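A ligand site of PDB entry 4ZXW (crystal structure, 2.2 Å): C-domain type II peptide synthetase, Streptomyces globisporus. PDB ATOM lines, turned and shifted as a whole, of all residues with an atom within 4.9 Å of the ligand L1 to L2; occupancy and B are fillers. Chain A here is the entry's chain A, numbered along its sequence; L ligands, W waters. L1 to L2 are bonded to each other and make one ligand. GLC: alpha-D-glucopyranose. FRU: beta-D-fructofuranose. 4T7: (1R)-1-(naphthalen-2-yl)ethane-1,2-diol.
Ile 48 touches the ligand L1 to L2.
CH2 of Trp 244 touches O4 of GLC L1, at 3.6 Å.
CG2 of Val 374 touches O6 of FRU L2, at 3.6 Å.
CE3 of Trp 394 touches O5 of FRU L2, at 3.6 Å.
His 415 touches the ligand L1 to L2.
O of Ala 423 touches C6 of FRU L2, 3.6 Å away.
Hydrophobic or aromatic side chains within 4 Å of the ligand L1 to L2: Ile 48, Val 49, Trp 244, Val 374 and Trp 394.
13 residues have an atom within 4 Å of the ligand L1 to L2: Ile 48, Val 49, Trp 244, Arg 246, Gln 372, Val 374, Trp 394, Arg 396, Ser 413, His 415, Ala 423, Gly 424 and Ser 425.
Along chain A the residues within 4 Å of the ligand L1 to L2 span positions 48 to 425.
Water W1 lies within hydrogen-bond range of O4 of GLC L1 (2.7 Å), OE2 of Glu 125 (2.7 Å) and NH2 of Arg 246 (3.2 Å).
Water W4 lies within hydrogen-bond range of an oxygen (O6) of GLC L1 (2.7 Å) and an oxygen (OAB) of 4T7 L3 (3.0 Å).
Water W3 lies within hydrogen-bond range of the guanidinium group (NE) of Arg 246 (2.7 Å), an oxygen (O3) of FRU L2 (2.7 Å) and the side-chain hydroxyl (OG) of Ser 425 (2.8 Å).
Water W5 bridges the backbone carbonyl oxygen (O) of His 47 and an oxygen (O4) of GLC L1.
Water W2 lies within hydrogen-bond range of O of Ile 393 (2.6 Å), O1 of FRU L2 (3.0 Å) and NZ of Lys 392 (3.3 Å).
The backbone carbonyl oxygen of Ser 413 sits at hydrogen-bond distance from the backbone NH of Ser 425, at 2.9 Å.
The side-chain amide nitrogen (NE2) of Gln 372 is in hydrogen-bond range of the side-chain hydroxyl (OG) of Ser 413, at 2.9 Å.
N of Ile 414 is in hydrogen-bond range of O of Gln 372 (3.0 Å).
OE1 of Glu 125 lies within salt-bridge range of NH2 of Arg 246, at 3.0 Å.
O of Ala 423 is in hydrogen-bond range of N of His 415.
N of Val 374 sits at hydrogen-bond distance from O of Ile 414 (2.8 Å).
O of Ser 404 is in hydrogen-bond range of NE1 of Trp 244 (2.9 Å).
The indole nitrogen (NE1) of Trp 244 lies within hydrogen-bond range of the side-chain carboxylate (OE2) of Glu 125 (3.5 Å).
An oxygen (O3) of GLC L1 lies within hydrogen-bond range of the backbone NH (N) of Val 49.
The backbone carbonyl oxygen of Val 49 sits at hydrogen-bond distance from an oxygen (O2) of GLC L1 (2.5 Å).
An oxygen (O6) of FRU L2 sits at hydrogen-bond distance from the side-chain hydroxyl (OG) of Ser 413, 2.6 Å away.
An oxygen (O4) of FRU L2 sits at hydrogen-bond distance from the side-chain hydroxyl (OG) of Ser 425 (2.8 Å).
The guanidinium group (NH1) of Arg 396 lies within hydrogen-bond range of an oxygen (O3) of FRU L2 (2.9 Å).
O of Gly 424 lies within hydrogen-bond range of O4 of FRU L2, at 3.1 Å.
The side-chain amide nitrogen of Gln 372 lies within hydrogen-bond range of an oxygen (O6) of GLC L1, at 3.3 Å.
O3 of FRU L2 lies within hydrogen-bond range of NE of Arg 246, at 3.3 Å.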
ATOM      1  N   HIS A  47     -24.524 -26.194 -14.413  1.00  0.00           N
ATOM      2  CA  HIS A  47     -23.414 -26.902 -13.782  1.00  0.00           C
ATOM      3  C   HIS A  47     -22.094 -26.265 -14.200  1.00  0.00           C
ATOM      4  O   HIS A  47     -22.053 -25.385 -15.059  1.00  0.00           O
ATOM      5  CB  HIS A  47     -23.427 -28.404 -14.134  1.00  0.00           C
ATOM      6  CG  HIS A  47     -23.772 -28.703 -15.570  1.00  0.00           C
ATOM      7  ND1 HIS A  47     -23.160 -28.081 -16.634  1.00  0.00           N
ATOM      8  CD2 HIS A  47     -24.677 -29.560 -16.109  1.00  0.00           C
ATOM      9  CE1 HIS A  47     -23.661 -28.543 -17.766  1.00  0.00           C
ATOM     10  NE2 HIS A  47     -24.580 -29.444 -17.473  1.00  0.00           N
ATOM     11  N   ILE A  48     -21.020 -26.727 -13.559  1.00  0.00           N
ATOM     12  CA  ILE A  48     -19.678 -26.224 -13.802  1.00  0.00           C
ATOM     13  C   ILE A  48     -18.800 -27.471 -13.955  1.00  0.00           C
ATOM     14  O   ILE A  48     -19.024 -28.463 -13.238  1.00  0.00           O
ATOM     15  CB  ILE A  48     -19.225 -25.283 -12.672  1.00  0.00           C
ATOM     16  CG1 ILE A  48     -17.803 -24.783 -12.920  1.00  0.00           C
ATOM     17  CG2 ILE A  48     -19.305 -26.000 -11.328  1.00  0.00           C
ATOM     18  CD1 ILE A  48     -17.374 -23.671 -11.971  1.00  0.00           C
ATOM     19  N   VAL A  49     -17.875 -27.456 -14.914  1.00  0.00           N
ATOM     20  CA  VAL A  49     -16.918 -28.549 -15.105  1.00  0.00           C
ATOM     21  C   VAL A  49     -15.477 -28.115 -14.797  1.00  0.00           C
ATOM     22  O   VAL A  49     -15.115 -26.950 -14.897  1.00  0.00           O
ATOM     23  CB  VAL A  49     -16.976 -29.109 -16.547  1.00  0.00           C
ATOM     24  CG1 VAL A  49     -18.373 -29.547 -16.858  1.00  0.00           C
ATOM     25  CG2 VAL A  49     -16.556 -28.065 -17.551  1.00  0.00           C
ATOM     26  N   GLY A  50     -14.672 -29.109 -14.433  1.00  0.00           N
ATOM     27  CA  GLY A  50     -13.232 -28.977 -14.341  1.00  0.00           C
ATOM     28  C   GLY A  50     -12.592 -30.229 -14.944  1.00  0.00           C
ATOM     29  O   GLY A  50     -13.059 -31.361 -14.714  1.00  0.00           O
ATOM     30  N   GLU A 125     -20.384 -31.673 -20.472  1.00  0.00           N
ATOM     31  CA  GLU A 125     -21.077 -30.421 -20.188  1.00  0.00           C
ATOM     32  C   GLU A 125     -22.432 -30.381 -20.901  1.00  0.00           C
ATOM     33  O   GLU A 125     -23.311 -29.624 -20.521  1.00  0.00           O
ATOM     34  CB  GLU A 125     -20.223 -29.197 -20.612  1.00  0.00           C
ATOM     35  CG  GLU A 125     -20.778 -27.840 -20.213  1.00  0.00           C
ATOM     36  CD  GLU A 125     -19.883 -26.640 -20.653  1.00  0.00           C
ATOM     37  OE1 GLU A 125     -18.626 -26.749 -20.557  1.00  0.00           O
ATOM     38  OE2 GLU A 125     -20.472 -25.587 -21.093  1.00  0.00           O
ATOM     39  N   TRP A 244     -21.457 -21.673 -26.093  1.00  0.00           N
ATOM     40  CA  TRP A 244     -20.196 -21.181 -25.536  1.00  0.00           C
ATOM     41  C   TRP A 244     -19.202 -21.138 -26.647  1.00  0.00           C
ATOM     42  O   TRP A 244     -18.883 -22.168 -27.227  1.00  0.00           O
ATOM     43  CB  TRP A 244     -19.676 -22.102 -24.431  1.00  0.00           C
ATOM     44  CG  TRP A 244     -20.567 -22.109 -23.241  1.00  0.00           C
ATOM     45  CD1 TRP A 244     -21.623 -22.906 -23.038  1.00  0.00           C
ATOM     46  CD2 TRP A 244     -20.476 -21.263 -22.081  1.00  0.00           C
ATOM     47  NE1 TRP A 244     -22.213 -22.643 -21.815  1.00  0.00           N
ATOM     48  CE2 TRP A 244     -21.525 -21.631 -21.215  1.00  0.00           C
ATOM     49  CE3 TRP A 244     -19.630 -20.238 -21.701  1.00  0.00           C
ATOM     50  CZ2 TRP A 244     -21.732 -21.018 -19.983  1.00  0.00           C
ATOM     51  CZ3 TRP A 244     -19.830 -19.627 -20.490  1.00  0.00           C
ATOM     52  CH2 TRP A 244     -20.873 -20.022 -19.637  1.00  0.00           C
ATOM     53  N   ARG A 246     -15.485 -20.465 -27.523  1.00  0.00           N
ATOM     54  CA  ARG A 246     -14.306 -20.547 -26.684  1.00  0.00           C
ATOM     55  C   ARG A 246     -13.165 -19.970 -27.471  1.00  0.00           C
ATOM     56  O   ARG A 246     -13.177 -20.023 -28.686  1.00  0.00           O
ATOM     57  CB  ARG A 246     -14.059 -22.000 -26.259  1.00  0.00           C
ATOM     58  CG  ARG A 246     -15.271 -22.553 -25.506  1.00  0.00           C
ATOM     59  CD  ARG A 246     -14.907 -23.592 -24.496  1.00  0.00           C
ATOM     60  NE  ARG A 246     -16.022 -23.863 -23.595  1.00  0.00           N
ATOM     61  CZ  ARG A 246     -16.938 -24.811 -23.791  1.00  0.00           C
ATOM     62  NH1 ARG A 246     -16.873 -25.597 -24.853  1.00  0.00           N
ATOM     63  NH2 ARG A 246     -17.919 -24.973 -22.926  1.00  0.00           N
ATOM     64  N   GLN A 372     -16.369 -11.334 -16.489  1.00  0.00           N
ATOM     65  CA  GLN A 372     -15.677 -11.858 -15.308  1.00  0.00           C
ATOM     66  C   GLN A 372     -14.298 -12.441 -15.576  1.00  0.00           C
ATOM     67  O   GLN A 372     -13.992 -12.926 -16.658  1.00  0.00           O
ATOM     68  CB  GLN A 372     -16.494 -12.951 -14.589  1.00  0.00           C
ATOM     69  CG  GLN A 372     -16.499 -14.288 -15.296  1.00  0.00           C
ATOM     70  CD  GLN A 372     -17.221 -15.410 -14.525  1.00  0.00           C
ATOM     71  OE1 GLN A 372     -17.915 -15.171 -13.530  1.00  0.00           O
ATOM     72  NE2 GLN A 372     -17.053 -16.648 -15.009  1.00  0.00           N
ATOM     73  N   VAL A 374     -12.254 -15.587 -13.917  1.00  0.00           N
ATOM     74  CA  VAL A 374     -12.364 -16.766 -13.078  1.00  0.00           C
ATOM     75  C   VAL A 374     -11.451 -16.686 -11.872  1.00  0.00           C
ATOM     76  O   VAL A 374     -10.250 -16.468 -12.028  1.00  0.00           O
ATOM     77  CB  VAL A 374     -12.057 -18.019 -13.874  1.00  0.00           C
ATOM     78  CG1 VAL A 374     -12.151 -19.261 -12.972  1.00  0.00           C
ATOM     79  CG2 VAL A 374     -12.973 -18.086 -15.068  1.00  0.00           C
ATOM     80  N   LYS A 392      -4.477 -28.566 -14.381  1.00  0.00           N
ATOM     81  CA  LYS A 392      -5.769 -28.137 -14.821  1.00  0.00           C
ATOM     82  C   LYS A 392      -5.744 -27.824 -16.309  1.00  0.00           C
ATOM     83  O   LYS A 392      -4.782 -27.287 -16.818  1.00  0.00           O
ATOM     84  CB  LYS A 392      -6.221 -26.914 -13.990  1.00  0.00           C
ATOM     85  CG  LYS A 392      -7.581 -26.333 -14.308  1.00  0.00           C
ATOM     86  CD  LYS A 392      -8.676 -27.363 -14.301  1.00  0.00           C
ATOM     87  CE  LYS A 392     -10.023 -26.774 -13.913  1.00  0.00           C
ATOM     88  NZ  LYS A 392     -10.328 -25.437 -14.509  1.00  0.00           N
ATOM     89  N   ILE A 393      -6.832 -28.143 -16.988  1.00  0.00           N
ATOM     90  CA  ILE A 393      -6.989 -27.782 -18.379  1.00  0.00           C
ATOM     91  C   ILE A 393      -7.819 -26.490 -18.435  1.00  0.00           C
ATOM     92  O   ILE A 393      -8.976 -26.495 -18.036  1.00  0.00           O
ATOM     93  CB  ILE A 393      -7.643 -28.907 -19.175  1.00  0.00           C
ATOM     94  CG1 ILE A 393      -6.691 -30.088 -19.255  1.00  0.00           C
ATOM     95  CG2 ILE A 393      -7.980 -28.469 -20.588  1.00  0.00           C
ATOM     96  CD1 ILE A 393      -7.371 -31.365 -19.714  1.00  0.00           C
ATOM     97  N   TRP A 394      -7.207 -25.385 -18.879  1.00  0.00           N
ATOM     98  CA  TRP A 394      -7.926 -24.109 -19.004  1.00  0.00           C
ATOM     99  C   TRP A 394      -8.301 -23.787 -20.428  1.00  0.00           C
ATOM    100  O   TRP A 394      -9.407 -23.322 -20.693  1.00  0.00           O
ATOM    101  CB  TRP A 394      -7.109 -22.937 -18.454  1.00  0.00           C
ATOM    102  CG  TRP A 394      -7.092 -22.907 -16.990  1.00  0.00           C
ATOM    103  CD1 TRP A 394      -6.020 -23.157 -16.184  1.00  0.00           C
ATOM    104  CD2 TRP A 394      -8.195 -22.616 -16.116  1.00  0.00           C
ATOM    105  NE1 TRP A 394      -6.388 -23.053 -14.860  1.00  0.00           N
ATOM    106  CE2 TRP A 394      -7.722 -22.719 -14.794  1.00  0.00           C
ATOM    107  CE3 TRP A 394      -9.552 -22.282 -16.331  1.00  0.00           C
ATOM    108  CZ2 TRP A 394      -8.536 -22.508 -13.684  1.00  0.00           C
ATOM    109  CZ3 TRP A 394     -10.362 -22.061 -15.231  1.00  0.00           C
ATOM    110  CH2 TRP A 394      -9.856 -22.184 -13.923  1.00  0.00           C
ATOM    111  N   ARG A 396      -9.614 -24.389 -23.716  1.00  0.00           N
ATOM    112  CA  ARG A 396     -10.448 -25.246 -24.532  1.00  0.00           C
ATOM    113  C   ARG A 396     -10.721 -24.471 -25.768  1.00  0.00           C
ATOM    114  O   ARG A 396     -11.196 -23.340 -25.692  1.00  0.00           O
ATOM    115  CB  ARG A 396     -11.762 -25.624 -23.843  1.00  0.00           C
ATOM    116  CG  ARG A 396     -11.585 -26.296 -22.549  1.00  0.00           C
ATOM    117  CD  ARG A 396     -12.855 -26.260 -21.755  1.00  0.00           C
ATOM    118  NE  ARG A 396     -13.987 -26.960 -22.343  1.00  0.00           N
ATOM    119  CZ  ARG A 396     -15.212 -26.908 -21.823  1.00  0.00           C
ATOM    120  NH1 ARG A 396     -15.449 -26.157 -20.745  1.00  0.00           N
ATOM    121  NH2 ARG A 396     -16.219 -27.581 -22.385  1.00  0.00           N
ATOM    122  N   SER A 404     -23.390 -25.581 -20.478  1.00  0.00           N
ATOM    123  CA  SER A 404     -23.877 -25.130 -19.168  1.00  0.00           C
ATOM    124  C   SER A 404     -24.773 -23.941 -19.333  1.00  0.00           C
ATOM    125  O   SER A 404     -24.513 -23.058 -20.165  1.00  0.00           O
ATOM    126  CB  SER A 404     -22.746 -24.750 -18.253  1.00  0.00           C
ATOM    127  OG  SER A 404     -21.875 -25.829 -18.075  1.00  0.00           O
ATOM    128  N   LEU A 411     -22.456 -14.062 -20.891  1.00  0.00           N
ATOM    129  CA  LEU A 411     -21.290 -14.114 -20.028  1.00  0.00           C
ATOM    130  C   LEU A 411     -19.973 -14.133 -20.812  1.00  0.00           C
ATOM    131  O   LEU A 411     -19.729 -15.001 -21.651  1.00  0.00           O
ATOM    132  CB  LEU A 411     -21.340 -15.324 -19.124  1.00  0.00           C
ATOM    133  CG  LEU A 411     -20.185 -15.463 -18.119  1.00  0.00           C
ATOM    134  CD1 LEU A 411     -20.269 -14.389 -17.114  1.00  0.00           C
ATOM    135  CD2 LEU A 411     -20.270 -16.791 -17.378  1.00  0.00           C
ATOM    136  N   SER A 413     -16.120 -14.689 -19.891  1.00  0.00           N
ATOM    137  CA  SER A 413     -15.388 -15.245 -18.787  1.00  0.00           C
ATOM    138  C   SER A 413     -13.964 -15.520 -19.264  1.00  0.00           C
ATOM    139  O   SER A 413     -13.754 -16.202 -20.242  1.00  0.00           O
ATOM    140  CB  SER A 413     -16.077 -16.509 -18.276  1.00  0.00           C
ATOM    141  OG  SER A 413     -15.306 -17.176 -17.268  1.00  0.00           O
ATOM    142  N   ILE A 414     -13.002 -14.972 -18.542  1.00  0.00           N
ATOM    143  CA  ILE A 414     -11.589 -15.149 -18.836  1.00  0.00           C
ATOM    144  C   ILE A 414     -10.893 -15.783 -17.649  1.00  0.00           C
ATOM    145  O   ILE A 414     -11.145 -15.394 -16.511  1.00  0.00           O
ATOM    146  CB  ILE A 414     -10.891 -13.800 -19.136  1.00  0.00           C
ATOM    147  CG1 ILE A 414     -11.625 -13.054 -20.238  1.00  0.00           C
ATOM    148  CG2 ILE A 414      -9.458 -14.049 -19.571  1.00  0.00           C
ATOM    149  CD1 ILE A 414     -11.785 -13.839 -21.488  1.00  0.00           C
ATOM    150  N   HIS A 415     -10.006 -16.744 -17.901  1.00  0.00           N
ATOM    151  CA  HIS A 415      -9.097 -17.194 -16.856  1.00  0.00           C
ATOM    152  C   HIS A 415      -7.733 -16.680 -17.260  1.00  0.00           C
ATOM    153  O   HIS A 415      -7.273 -16.928 -18.374  1.00  0.00           O
ATOM    154  CB  HIS A 415      -9.044 -18.719 -16.670  1.00  0.00           C
ATOM    155  CG  HIS A 415      -7.984 -19.139 -15.701  1.00  0.00           C
ATOM    156  ND1 HIS A 415      -6.734 -19.559 -16.094  1.00  0.00           N
ATOM    157  CD2 HIS A 415      -7.964 -19.103 -14.337  1.00  0.00           C
ATOM    158  CE1 HIS A 415      -5.997 -19.797 -15.015  1.00  0.00           C
ATOM    159  NE2 HIS A 415      -6.713 -19.515 -13.943  1.00  0.00           N
ATOM    160  N   ALA A 423      -7.469 -17.964 -21.273  1.00  0.00           N
ATOM    161  CA  ALA A 423      -8.475 -18.801 -21.874  1.00  0.00           C
ATOM    162  C   ALA A 423      -9.839 -18.166 -21.642  1.00  0.00           C
ATOM    163  O   ALA A 423     -10.223 -17.895 -20.510  1.00  0.00           O
ATOM    164  CB  ALA A 423      -8.441 -20.159 -21.255  1.00  0.00           C
ATOM    165  N   GLY A 424     -10.609 -17.968 -22.703  1.00  0.00           N
ATOM    166  CA  GLY A 424     -11.876 -17.293 -22.553  1.00  0.00           C
ATOM    167  C   GLY A 424     -13.059 -17.971 -23.176  1.00  0.00           C
ATOM    168  O   GLY A 424     -12.929 -18.822 -24.067  1.00  0.00           O
ATOM    169  N   SER A 425     -14.246 -17.558 -22.717  1.00  0.00           N
ATOM    170  CA  SER A 425     -15.515 -17.985 -23.286  1.00  0.00           C
ATOM    171  C   SER A 425     -16.468 -16.825 -23.381  1.00  0.00           C
ATOM    172  O   SER A 425     -16.540 -15.998 -22.486  1.00  0.00           O
ATOM    173  CB  SER A 425     -16.183 -19.050 -22.452  1.00  0.00           C
ATOM    174  OG  SER A 425     -15.537 -20.261 -22.567  1.00  0.00           O
HETATM  175  C1  GLC L   1     -14.853 -22.743 -16.841  1.00  0.00           C
HETATM  176  C2  GLC L   1     -15.772 -23.869 -16.392  1.00  0.00           C
HETATM  177  C3  GLC L   1     -17.106 -23.887 -17.123  1.00  0.00           C
HETATM  178  C4  GLC L   1     -17.733 -22.510 -17.020  1.00  0.00           C
HETATM  179  C5  GLC L   1     -16.753 -21.429 -17.518  1.00  0.00           C
HETATM  180  C6  GLC L   1     -17.402 -20.043 -17.352  1.00  0.00           C
HETATM  181  O2  GLC L   1     -15.138 -25.111 -16.631  1.00  0.00           O
HETATM  182  O3  GLC L   1     -17.951 -24.841 -16.456  1.00  0.00           O
HETATM  183  O4  GLC L   1     -18.941 -22.486 -17.793  1.00  0.00           O
HETATM  184  O5  GLC L   1     -15.511 -21.483 -16.790  1.00  0.00           O
HETATM  185  O6  GLC L   1     -17.512 -19.763 -15.963  1.00  0.00           O
HETATM  186  C1  FRU L   2     -12.410 -24.204 -18.320  1.00  0.00           C
HETATM  187  C2  FRU L   2     -13.201 -22.928 -18.632  1.00  0.00           C
HETATM  188  C3  FRU L   2     -13.411 -22.635 -20.109  1.00  0.00           C
HETATM  189  C4  FRU L   2     -13.385 -21.108 -20.339  1.00  0.00           C
HETATM  190  C5  FRU L   2     -12.479 -20.701 -19.186  1.00  0.00           C
HETATM  191  C6  FRU L   2     -12.933 -19.348 -18.632  1.00  0.00           C
HETATM  192  O1  FRU L   2     -13.203 -25.383 -18.378  1.00  0.00           O
HETATM  193  O2  FRU L   2     -14.546 -23.019 -18.191  1.00  0.00           O
HETATM  194  O3  FRU L   2     -14.122 -23.581 -20.922  1.00  0.00           O
HETATM  195  O4  FRU L   2     -12.932 -20.642 -21.613  1.00  0.00           O
HETATM  196  O5  FRU L   2     -12.545 -21.732 -18.161  1.00  0.00           O
HETATM  197  O6  FRU L   2     -14.304 -19.448 -18.161  1.00  0.00           O
HETATM  198  CAI 4T7 L   3     -24.063 -15.948 -15.165  1.00  0.00           C
HETATM  199  CAM 4T7 L   3     -25.060 -14.980 -15.339  1.00  0.00           C
HETATM  200  CAG 4T7 L   3     -25.031 -14.143 -16.455  1.00  0.00           C
HETATM  201  CAD 4T7 L   3     -26.040 -13.187 -16.661  1.00  0.00           C
HETATM  202  CAC 4T7 L   3     -27.084 -13.078 -15.750  1.00  0.00           C
HETATM  203  CAF 4T7 L   3     -27.118 -13.923 -14.635  1.00  0.00           C
HETATM  204  CAL 4T7 L   3     -26.115 -14.885 -14.440  1.00  0.00           C
HETATM  205  CAH 4T7 L   3     -26.128 -15.732 -13.337  1.00  0.00           C
HETATM  206  CAE 4T7 L   3     -25.110 -16.666 -13.160  1.00  0.00           C
HETATM  207  CAK 4T7 L   3     -24.069 -16.822 -14.065  1.00  0.00           C
HETATM  208  CAN 4T7 L   3     -23.035 -17.818 -13.836  1.00  0.00           C
HETATM  209  OAB 4T7 L   3     -22.604 -18.541 -15.012  1.00  0.00           O
HETATM  210  CAJ 4T7 L   3     -21.767 -17.220 -13.186  1.00  0.00           C
HETATM  211  OAA 4T7 L   3     -20.772 -18.238 -12.967  1.00  0.00           O
HETATM  212  O   HOH W   1     -19.006 -23.468 -20.301  1.00  0.00           O
HETATM  213  O   HOH W   2     -11.244 -27.256 -17.053  1.00  0.00           O
HETATM  214  O   HOH W   3     -16.630 -22.515 -21.279  1.00  0.00           O
HETATM  215  O   HOH W   4     -20.098 -20.258 -15.233  1.00  0.00           O
HETATM  216  O   HOH W   5     -20.884 -23.009 -15.794  1.00  0.00           O
HETATM  217  O   HOH W   6     -15.905 -20.735 -13.970  1.00  0.00           O
HETATM  218  O   HOH W   7     -11.276 -21.695 -23.080  1.00  0.00           O
